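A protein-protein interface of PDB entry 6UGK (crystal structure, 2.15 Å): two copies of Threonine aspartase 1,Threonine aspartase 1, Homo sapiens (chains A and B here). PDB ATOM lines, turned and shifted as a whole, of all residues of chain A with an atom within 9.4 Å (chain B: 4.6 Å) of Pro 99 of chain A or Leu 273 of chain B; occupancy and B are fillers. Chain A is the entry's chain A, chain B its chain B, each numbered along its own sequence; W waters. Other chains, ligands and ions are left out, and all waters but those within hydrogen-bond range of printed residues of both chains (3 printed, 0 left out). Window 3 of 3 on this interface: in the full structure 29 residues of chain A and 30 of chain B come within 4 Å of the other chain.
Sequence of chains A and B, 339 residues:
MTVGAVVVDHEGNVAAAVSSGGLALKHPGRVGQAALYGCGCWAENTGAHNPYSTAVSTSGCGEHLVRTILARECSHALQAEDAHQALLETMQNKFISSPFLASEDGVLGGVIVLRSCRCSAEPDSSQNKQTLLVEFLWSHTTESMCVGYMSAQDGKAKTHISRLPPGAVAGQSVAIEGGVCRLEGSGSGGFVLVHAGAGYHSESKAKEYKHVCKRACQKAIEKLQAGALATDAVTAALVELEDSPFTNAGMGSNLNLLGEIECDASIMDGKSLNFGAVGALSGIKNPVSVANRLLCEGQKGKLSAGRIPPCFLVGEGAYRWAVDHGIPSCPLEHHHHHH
The side-chain amide oxygen (OD1) of Asn 274 of chain B is in hydrogen-bond range of the guanidinium group (NH2) of Arg 67 of chain A (2.8 Å).
The backbone NH of Asp 269 of chain B lies within hydrogen-bond range of the backbone carbonyl oxygen of Asn 274 of chain B (3.0 Å). N of Asn 274 of chain B sits close to OG of Ser 272 of chain B, 3.2 Å away. The side-chain hydroxyl (OG) of Ser 98 of chain A lies within hydrogen-bond range of the backbone NH (N) of Phe 100 of chain A, at 3.0 Å. The side-chain carboxylate of Glu 63 of chain A lies within salt-bridge range of the guanidinium group of Arg 67 of chain A. The backbone NH (N) of Ala 43 of chain B is in hydrogen-bond range of the side-chain sulfur (SD) of Met 268 of chain B (3.5 Å).
Phe 275 of chain B touches Arg 67 of chain A (N to NH2, 3.7 Å). Pro 99 of chain A touches Leu 273 of chain B. CZ of Phe 100 of chain A touches OE1 of Glu 44 of chain B (3.7 Å). Met 268 of chain B touches Phe 100 of chain A (CE to CE2, 3.8 Å). Phe 100 of chain A touches Leu 273 of chain B.
Pro 99 of chain A touches just one residue of chain B: Leu 273 (3.6 Å). Leu 273 of chain B touches just these residues of chain A: Pro 99 and Phe 100. No residue of chain A comes within 4 Å of Gly 270 of chain B. No residue of chain A comes within 4 Å of Ser 272 of chain B. Printed residues of chain A within 4 Å of Asn 274 of chain B: Arg 67 (2.8 Å). Printed residues of chain B within 4 Å of Phe 100 of chain A: Glu 44, Met 268 and Leu 273. The nearest printed residue of chain B that does not touch Pro 99 of chain A is Ser 272 of chain B (5.4 Å). The nearest residue of chain A that does not touch Leu 273 of chain B is Arg 67 of chain A (4.04 Å). The nearest printed residue of chain A that does not touch Met 268 of chain B is Arg 67 of chain A (6.4 Å).
Of the 10 printed residues of chain B, 5 touch a printed residue of chain A. Along chain B the printed residues that touch a printed residue of chain A span positions 44 to 275. Of the 18 printed residues of chain A, 3 touch a printed residue of chain B. Hydrophobic or aromatic side chains of chain A within 4 Å of the printed part of chain B: Phe 100. Among the printed residues, 6 pairs touch across the chains.
No position is printed for both chains. Of the 6 pairs that touch across the chains among the printed residues, none has its exchanged pair printed and touching as well.
Water W3 lies within hydrogen-bond range of the backbone carbonyl oxygen of Leu 273 of chain B (2.5 Å) and the guanidinium group of Arg 67 of chain A (3.2 Å). Water W1 lies within hydrogen-bond range of O of Phe 100 of chain A (2.7 Å), O of Leu 273 of chain B (3.3 Å) and NH2 of Arg 67 of chain A (3.3 Å). Water W2 lies within hydrogen-bond range of the side-chain amide nitrogen (ND2) of Asn 274 of chain B, the backbone carbonyl oxygen (O) of Ser 272 of chain B and the guanidinium group (NH2) of Arg 67 of chain A.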
ATOM      1  N   GLU A  63      -3.065 -33.358  12.290  1.00  0.00           N
ATOM      2  CA  GLU A  63      -4.171 -32.636  11.667  1.00  0.00           C
ATOM      3  C   GLU A  63      -3.696 -31.352  11.003  1.00  0.00           C
ATOM      4  O   GLU A  63      -4.204 -30.981   9.942  1.00  0.00           O
ATOM      5  CB  GLU A  63      -5.262 -32.329  12.694  1.00  0.00           C
ATOM      6  CG  GLU A  63      -5.980 -33.556  13.251  1.00  0.00           C
ATOM      7  CD  GLU A  63      -6.869 -34.272  12.232  1.00  0.00           C
ATOM      8  OE1 GLU A  63      -6.668 -35.492  12.014  1.00  0.00           O
ATOM      9  OE2 GLU A  63      -7.774 -33.619  11.661  1.00  0.00           O
ATOM     10  N   VAL A  66      -2.119 -32.317   7.709  1.00  0.00           N
ATOM     11  CA  VAL A  66      -3.099 -32.786   6.728  1.00  0.00           C
ATOM     12  C   VAL A  66      -3.839 -31.614   6.099  1.00  0.00           C
ATOM     13  O   VAL A  66      -3.945 -31.524   4.872  1.00  0.00           O
ATOM     14  CB  VAL A  66      -4.095 -33.777   7.362  1.00  0.00           C
ATOM     15  CG1 VAL A  66      -5.202 -34.137   6.359  1.00  0.00           C
ATOM     16  CG2 VAL A  66      -3.381 -35.036   7.846  1.00  0.00           C
ATOM     17  N   ARG A  67      -4.381 -30.711   6.928  1.00  0.00           N
ATOM     18  CA  ARG A  67      -5.292 -29.699   6.399  1.00  0.00           C
ATOM     19  C   ARG A  67      -4.586 -28.770   5.413  1.00  0.00           C
ATOM     20  O   ARG A  67      -5.225 -28.233   4.508  1.00  0.00           O
ATOM     21  CB  ARG A  67      -5.921 -28.879   7.531  1.00  0.00           C
ATOM     22  CG  ARG A  67      -6.654 -29.676   8.633  1.00  0.00           C
ATOM     23  CD  ARG A  67      -7.684 -30.681   8.128  1.00  0.00           C
ATOM     24  NE  ARG A  67      -8.375 -31.345   9.242  1.00  0.00           N
ATOM     25  CZ  ARG A  67      -9.618 -31.074   9.640  1.00  0.00           C
ATOM     26  NH1 ARG A  67     -10.146 -31.726  10.672  1.00  0.00           N
ATOM     27  NH2 ARG A  67     -10.338 -30.158   9.003  1.00  0.00           N
ATOM     28  N   THR A  68      -3.274 -28.601   5.554  1.00  0.00           N
ATOM     29  CA  THR A  68      -2.483 -27.751   4.682  1.00  0.00           C
ATOM     30  C   THR A  68      -1.720 -28.525   3.613  1.00  0.00           C
ATOM     31  O   THR A  68      -1.019 -27.903   2.818  1.00  0.00           O
ATOM     32  CB  THR A  68      -1.497 -26.936   5.526  1.00  0.00           C
ATOM     33  OG1 THR A  68      -0.676 -27.835   6.286  1.00  0.00           O
ATOM     34  CG2 THR A  68      -2.240 -26.026   6.498  1.00  0.00           C
ATOM     35  N   GLN A  92       5.538 -19.978   7.039  1.00  0.00           N
ATOM     36  CA  GLN A  92       4.854 -18.829   7.615  1.00  0.00           C
ATOM     37  C   GLN A  92       3.444 -18.686   7.065  1.00  0.00           C
ATOM     38  O   GLN A  92       2.488 -18.502   7.822  1.00  0.00           O
ATOM     39  CB  GLN A  92       5.665 -17.554   7.332  1.00  0.00           C
ATOM     40  CG  GLN A  92       6.836 -17.379   8.283  1.00  0.00           C
ATOM     41  CD  GLN A  92       7.741 -16.243   7.882  1.00  0.00           C
ATOM     42  OE1 GLN A  92       7.823 -15.882   6.704  1.00  0.00           O
ATOM     43  NE2 GLN A  92       8.432 -15.675   8.858  1.00  0.00           N
ATOM     44  N   ASN A  93       3.300 -18.739   5.740  1.00  0.00           N
ATOM     45  CA  ASN A  93       2.069 -18.334   5.075  1.00  0.00           C
ATOM     46  C   ASN A  93       1.149 -19.507   4.767  1.00  0.00           C
ATOM     47  O   ASN A  93      -0.074 -19.363   4.865  1.00  0.00           O
ATOM     48  CB  ASN A  93       2.386 -17.593   3.770  1.00  0.00           C
ATOM     49  CG  ASN A  93       3.228 -16.340   3.986  1.00  0.00           C
ATOM     50  OD1 ASN A  93       2.970 -15.540   4.895  1.00  0.00           O
ATOM     51  ND2 ASN A  93       4.239 -16.161   3.140  1.00  0.00           N
ATOM     52  N   LYS A  94       1.705 -20.656   4.365  1.00  0.00           N
ATOM     53  CA  LYS A  94       0.898 -21.820   4.005  1.00  0.00           C
ATOM     54  C   LYS A  94       0.703 -22.771   5.173  1.00  0.00           C
ATOM     55  O   LYS A  94      -0.042 -23.749   5.045  1.00  0.00           O
ATOM     56  CB  LYS A  94       1.529 -22.589   2.823  1.00  0.00           C
ATOM     57  CG  LYS A  94       1.734 -21.727   1.546  1.00  0.00           C
ATOM     58  CD  LYS A  94       0.399 -21.197   1.041  1.00  0.00           C
ATOM     59  CE  LYS A  94       0.315 -21.239  -0.487  1.00  0.00           C
ATOM     60  NZ  LYS A  94      -1.090 -21.190  -0.989  1.00  0.00           N
ATOM     61  N   PHE A  95       1.351 -22.510   6.301  1.00  0.00           N
ATOM     62  CA  PHE A  95       1.210 -23.372   7.463  1.00  0.00           C
ATOM     63  C   PHE A  95       0.671 -22.538   8.625  1.00  0.00           C
ATOM     64  O   PHE A  95      -0.542 -22.544   8.870  1.00  0.00           O
ATOM     65  CB  PHE A  95       2.555 -24.047   7.770  1.00  0.00           C
ATOM     66  CG  PHE A  95       2.473 -25.175   8.761  1.00  0.00           C
ATOM     67  CD1 PHE A  95       1.555 -26.209   8.597  1.00  0.00           C
ATOM     68  CD2 PHE A  95       3.333 -25.208   9.853  1.00  0.00           C
ATOM     69  CE1 PHE A  95       1.490 -27.255   9.513  1.00  0.00           C
ATOM     70  CE2 PHE A  95       3.279 -26.249  10.764  1.00  0.00           C
ATOM     71  CZ  PHE A  95       2.348 -27.272  10.594  1.00  0.00           C
ATOM     72  N   ILE A  96       1.530 -21.763   9.300  1.00  0.00           N
ATOM     73  CA  ILE A  96       1.090 -20.973  10.459  1.00  0.00           C
ATOM     74  C   ILE A  96      -0.138 -20.135  10.123  1.00  0.00           C
ATOM     75  O   ILE A  96      -1.110 -20.090  10.889  1.00  0.00           O
ATOM     76  CB  ILE A  96       2.237 -20.088  10.981  1.00  0.00           C
ATOM     77  CG1 ILE A  96       3.296 -20.940  11.676  1.00  0.00           C
ATOM     78  CG2 ILE A  96       1.706 -18.973  11.942  1.00  0.00           C
ATOM     79  CD1 ILE A  96       4.469 -20.119  12.208  1.00  0.00           C
ATOM     80  N   SER A  97      -0.112 -19.438   8.985  1.00  0.00           N
ATOM     81  CA  SER A  97      -1.195 -18.531   8.610  1.00  0.00           C
ATOM     82  C   SER A  97      -2.189 -19.146   7.621  1.00  0.00           C
ATOM     83  O   SER A  97      -2.908 -18.409   6.950  1.00  0.00           O
ATOM     84  CB  SER A  97      -0.627 -17.235   8.018  1.00  0.00           C
ATOM     85  OG  SER A  97       0.053 -16.505   9.010  1.00  0.00           O
ATOM     86  N   SER A  98      -2.253 -20.460   7.500  1.00  0.00           N
ATOM     87  CA  SER A  98      -3.244 -21.031   6.592  1.00  0.00           C
ATOM     88  C   SER A  98      -4.650 -20.720   7.100  1.00  0.00           C
ATOM     89  O   SER A  98      -4.918 -20.880   8.299  1.00  0.00           O
ATOM     90  CB  SER A  98      -3.063 -22.544   6.470  1.00  0.00           C
ATOM     91  OG  SER A  98      -4.053 -23.088   5.621  1.00  0.00           O
ATOM     92  N   PRO A  99      -5.569 -20.258   6.242  1.00  0.00           N
ATOM     93  CA  PRO A  99      -6.981 -20.221   6.657  1.00  0.00           C
ATOM     94  C   PRO A  99      -7.519 -21.593   7.050  1.00  0.00           C
ATOM     95  O   PRO A  99      -8.474 -21.666   7.833  1.00  0.00           O
ATOM     96  CB  PRO A  99      -7.709 -19.655   5.426  1.00  0.00           C
ATOM     97  CG  PRO A  99      -6.726 -19.743   4.289  1.00  0.00           C
ATOM     98  CD  PRO A  99      -5.364 -19.638   4.922  1.00  0.00           C
ATOM     99  N   PHE A 100      -6.923 -22.678   6.552  1.00  0.00           N
ATOM    100  CA  PHE A 100      -7.325 -24.024   6.944  1.00  0.00           C
ATOM    101  C   PHE A 100      -7.035 -24.328   8.409  1.00  0.00           C
ATOM    102  O   PHE A 100      -7.521 -25.343   8.923  1.00  0.00           O
ATOM    103  CB  PHE A 100      -6.642 -25.046   6.016  1.00  0.00           C
ATOM    104  CG  PHE A 100      -7.107 -24.931   4.606  1.00  0.00           C
ATOM    105  CD1 PHE A 100      -6.567 -23.969   3.765  1.00  0.00           C
ATOM    106  CD2 PHE A 100      -8.150 -25.713   4.143  1.00  0.00           C
ATOM    107  CE1 PHE A 100      -7.044 -23.805   2.465  1.00  0.00           C
ATOM    108  CE2 PHE A 100      -8.620 -25.563   2.845  1.00  0.00           C
ATOM    109  CZ  PHE A 100      -8.063 -24.606   2.006  1.00  0.00           C
ATOM    110  N   LEU A 101      -6.275 -23.474   9.098  1.00  0.00           N
ATOM    111  CA  LEU A 101      -5.975 -23.675  10.511  1.00  0.00           C
ATOM    112  C   LEU A 101      -6.292 -22.440  11.342  1.00  0.00           C
ATOM    113  O   LEU A 101      -5.791 -22.315  12.467  1.00  0.00           O
ATOM    114  CB  LEU A 101      -4.506 -24.064  10.697  1.00  0.00           C
ATOM    115  CG  LEU A 101      -4.037 -25.299   9.928  1.00  0.00           C
ATOM    116  CD1 LEU A 101      -2.515 -25.486  10.033  1.00  0.00           C
ATOM    117  CD2 LEU A 101      -4.771 -26.512  10.448  1.00  0.00           C
ATOM    118  N   ALA A 102      -7.121 -21.527  10.820  1.00  0.00           N
ATOM    119  CA  ALA A 102      -7.330 -20.242  11.490  1.00  0.00           C
ATOM    120  C   ALA A 102      -7.987 -20.396  12.857  1.00  0.00           C
ATOM    121  O   ALA A 102      -7.840 -19.508  13.706  1.00  0.00           O
ATOM    122  CB  ALA A 102      -8.164 -19.308  10.610  1.00  0.00           C
ATOM    123  N   SER A 103      -8.692 -21.508  13.098  1.00  0.00           N
ATOM    124  CA  SER A 103      -9.281 -21.740  14.417  1.00  0.00           C
ATOM    125  C   SER A 103      -8.251 -22.177  15.448  1.00  0.00           C
ATOM    126  O   SER A 103      -8.547 -22.164  16.647  1.00  0.00           O
ATOM    127  CB  SER A 103     -10.377 -22.805  14.341  1.00  0.00           C
ATOM    128  OG  SER A 103     -11.415 -22.421  13.461  1.00  0.00           O
ATOM    129  N   GLU A 104      -7.065 -22.584  15.019  1.00  0.00           N
ATOM    130  CA  GLU A 104      -6.108 -23.186  15.934  1.00  0.00           C
ATOM    131  C   GLU A 104      -5.367 -22.122  16.732  1.00  0.00           C
ATOM    132  O   GLU A 104      -4.975 -21.078  16.200  1.00  0.00           O
ATOM    133  CB  GLU A 104      -5.114 -24.051  15.166  1.00  0.00           C
ATOM    134  CG  GLU A 104      -5.772 -25.187  14.407  1.00  0.00           C
ATOM    135  CD  GLU A 104      -6.724 -25.969  15.280  1.00  0.00           C
ATOM    136  OE1 GLU A 104      -6.298 -26.426  16.366  1.00  0.00           O
ATOM    137  OE2 GLU A 104      -7.904 -26.107  14.892  1.00  0.00           O
ATOM    138  N   VAL A 107       0.102 -23.470  15.622  1.00  0.00           N
ATOM    139  CA  VAL A 107       0.203 -24.435  14.527  1.00  0.00           C
ATOM    140  C   VAL A 107       1.559 -25.113  14.652  1.00  0.00           C
ATOM    141  O   VAL A 107       2.598 -24.439  14.652  1.00  0.00           O
ATOM    142  CB  VAL A 107       0.043 -23.758  13.157  1.00  0.00           C
ATOM    143  CG1 VAL A 107       0.356 -24.730  12.045  1.00  0.00           C
ATOM    144  CG2 VAL A 107      -1.359 -23.182  13.008  1.00  0.00           C
ATOM    145  N   ALA B  43     -14.067 -28.345  -0.990  1.00  0.00           N
ATOM    146  CA  ALA B  43     -14.972 -27.202  -0.911  1.00  0.00           C
ATOM    147  C   ALA B  43     -14.285 -26.041  -0.195  1.00  0.00           C
ATOM    148  O   ALA B  43     -13.707 -26.215   0.880  1.00  0.00           O
ATOM    149  CB  ALA B  43     -16.285 -27.584  -0.212  1.00  0.00           C
ATOM    150  N   GLU B  44     -14.328 -24.860  -0.803  1.00  0.00           N
ATOM    151  CA  GLU B  44     -13.562 -23.734  -0.268  1.00  0.00           C
ATOM    152  C   GLU B  44     -14.287 -22.443  -0.621  1.00  0.00           C
ATOM    153  O   GLU B  44     -14.393 -22.102  -1.803  1.00  0.00           O
ATOM    154  CB  GLU B  44     -12.136 -23.748  -0.822  1.00  0.00           C
ATOM    155  CG  GLU B  44     -11.247 -22.618  -0.340  1.00  0.00           C
ATOM    156  CD  GLU B  44      -9.802 -22.769  -0.821  1.00  0.00           C
ATOM    157  OE1 GLU B  44      -9.435 -23.839  -1.377  1.00  0.00           O
ATOM    158  OE2 GLU B  44      -9.028 -21.805  -0.642  1.00  0.00           O
ATOM    159  N   MET B 268     -16.558 -32.132   2.619  1.00  0.00           N
ATOM    160  CA  MET B 268     -15.821 -30.934   2.982  1.00  0.00           C
ATOM    161  C   MET B 268     -16.778 -29.756   3.018  1.00  0.00           C
ATOM    162  O   MET B 268     -17.733 -29.696   2.232  1.00  0.00           O
ATOM    163  CB  MET B 268     -14.666 -30.672   2.005  1.00  0.00           C
ATOM    164  CG  MET B 268     -13.723 -29.557   2.469  1.00  0.00           C
ATOM    165  SD  MET B 268     -12.180 -29.693   1.603  1.00  0.00           S
ATOM    166  CE  MET B 268     -11.261 -28.277   2.271  1.00  0.00           C
ATOM    167  N   ASP B 269     -16.534 -28.837   3.953  1.00  0.00           N
ATOM    168  CA  ASP B 269     -17.371 -27.658   4.144  1.00  0.00           C
ATOM    169  C   ASP B 269     -16.592 -26.416   3.716  1.00  0.00           C
ATOM    170  O   ASP B 269     -15.519 -26.148   4.258  1.00  0.00           O
ATOM    171  CB  ASP B 269     -17.786 -27.539   5.604  1.00  0.00           C
ATOM    172  CG  ASP B 269     -18.637 -26.336   5.849  1.00  0.00           C
ATOM    173  OD1 ASP B 269     -19.601 -26.150   5.080  1.00  0.00           O
ATOM    174  OD2 ASP B 269     -18.338 -25.578   6.792  1.00  0.00           O
ATOM    175  N   GLY B 270     -17.124 -25.663   2.753  1.00  0.00           N
ATOM    176  CA  GLY B 270     -16.366 -24.537   2.228  1.00  0.00           C
ATOM    177  C   GLY B 270     -16.247 -23.371   3.192  1.00  0.00           C
ATOM    178  O   GLY B 270     -15.299 -22.580   3.107  1.00  0.00           O
ATOM    179  N   LYS B 271     -17.194 -23.235   4.117  1.00  0.00           N
ATOM    180  CA  LYS B 271     -17.144 -22.090   5.024  1.00  0.00           C
ATOM    181  C   LYS B 271     -16.130 -22.304   6.144  1.00  0.00           C
ATOM    182  O   LYS B 271     -15.265 -21.455   6.376  1.00  0.00           O
ATOM    183  CB  LYS B 271     -18.531 -21.815   5.598  1.00  0.00           C
ATOM    184  CG  LYS B 271     -18.616 -20.553   6.469  1.00  0.00           C
ATOM    185  CD  LYS B 271     -20.053 -20.320   6.950  1.00  0.00           C
ATOM    186  CE  LYS B 271     -20.109 -19.223   7.986  1.00  0.00           C
ATOM    187  NZ  LYS B 271     -19.236 -18.110   7.524  1.00  0.00           N
ATOM    188  N   SER B 272     -16.216 -23.427   6.846  1.00  0.00           N
ATOM    189  CA  SER B 272     -15.285 -23.723   7.924  1.00  0.00           C
ATOM    190  C   SER B 272     -14.002 -24.388   7.445  1.00  0.00           C
ATOM    191  O   SER B 272     -13.044 -24.466   8.218  1.00  0.00           O
ATOM    192  CB  SER B 272     -15.953 -24.640   8.962  1.00  0.00           C
ATOM    193  OG  SER B 272     -16.230 -25.924   8.397  1.00  0.00           O
ATOM    194  N   LEU B 273     -13.975 -24.895   6.211  1.00  0.00           N
ATOM    195  CA  LEU B 273     -12.879 -25.678   5.650  1.00  0.00           C
ATOM    196  C   LEU B 273     -12.720 -27.028   6.354  1.00  0.00           C
ATOM    197  O   LEU B 273     -11.754 -27.744   6.096  1.00  0.00           O
ATOM    198  CB  LEU B 273     -11.554 -24.905   5.663  1.00  0.00           C
ATOM    199  CG  LEU B 273     -11.567 -23.622   4.800  1.00  0.00           C
ATOM    200  CD1 LEU B 273     -10.266 -22.821   4.901  1.00  0.00           C
ATOM    201  CD2 LEU B 273     -11.889 -23.917   3.326  1.00  0.00           C
ATOM    202  N   ASN B 274     -13.658 -27.409   7.213  1.00  0.00           N
ATOM    203  CA  ASN B 274     -13.521 -28.673   7.913  1.00  0.00           C
ATOM    204  C   ASN B 274     -13.892 -29.831   6.998  1.00  0.00           C
ATOM    205  O   ASN B 274     -14.490 -29.654   5.937  1.00  0.00           O
ATOM    206  CB  ASN B 274     -14.372 -28.699   9.174  1.00  0.00           C
ATOM    207  CG  ASN B 274     -13.642 -29.331  10.339  1.00  0.00           C
ATOM    208  OD1 ASN B 274     -12.879 -30.306  10.173  1.00  0.00           O
ATOM    209  ND2 ASN B 274     -13.851 -28.773  11.527  1.00  0.00           N
ATOM    210  N   PHE B 275     -13.545 -31.034   7.452  1.00  0.00           N
ATOM    211  CA  PHE B 275     -13.467 -32.226   6.620  1.00  0.00           C
ATOM    212  C   PHE B 275     -13.810 -33.440   7.472  1.00  0.00           C
ATOM    213  O   PHE B 275     -13.490 -33.475   8.665  1.00  0.00           O
ATOM    214  CB  PHE B 275     -12.054 -32.353   6.040  1.00  0.00           C
ATOM    215  CG  PHE B 275     -11.831 -33.584   5.204  1.00  0.00           C
ATOM    216  CD1 PHE B 275     -12.268 -33.631   3.884  1.00  0.00           C
ATOM    217  CD2 PHE B 275     -11.130 -34.670   5.715  1.00  0.00           C
ATOM    218  CE1 PHE B 275     -12.034 -34.755   3.099  1.00  0.00           C
ATOM    219  CE2 PHE B 275     -10.890 -35.798   4.935  1.00  0.00           C
ATOM    220  CZ  PHE B 275     -11.346 -35.839   3.631  1.00  0.00           C
HETATM  221  O   HOH W   1      -9.578 -26.957   8.464  1.00  0.00           O
HETATM  222  O   HOH W   2     -11.578 -27.056  10.025  1.00  0.00           O
HETATM  223  O   HOH W   3      -9.400 -28.686   6.268  1.00  0.00           O
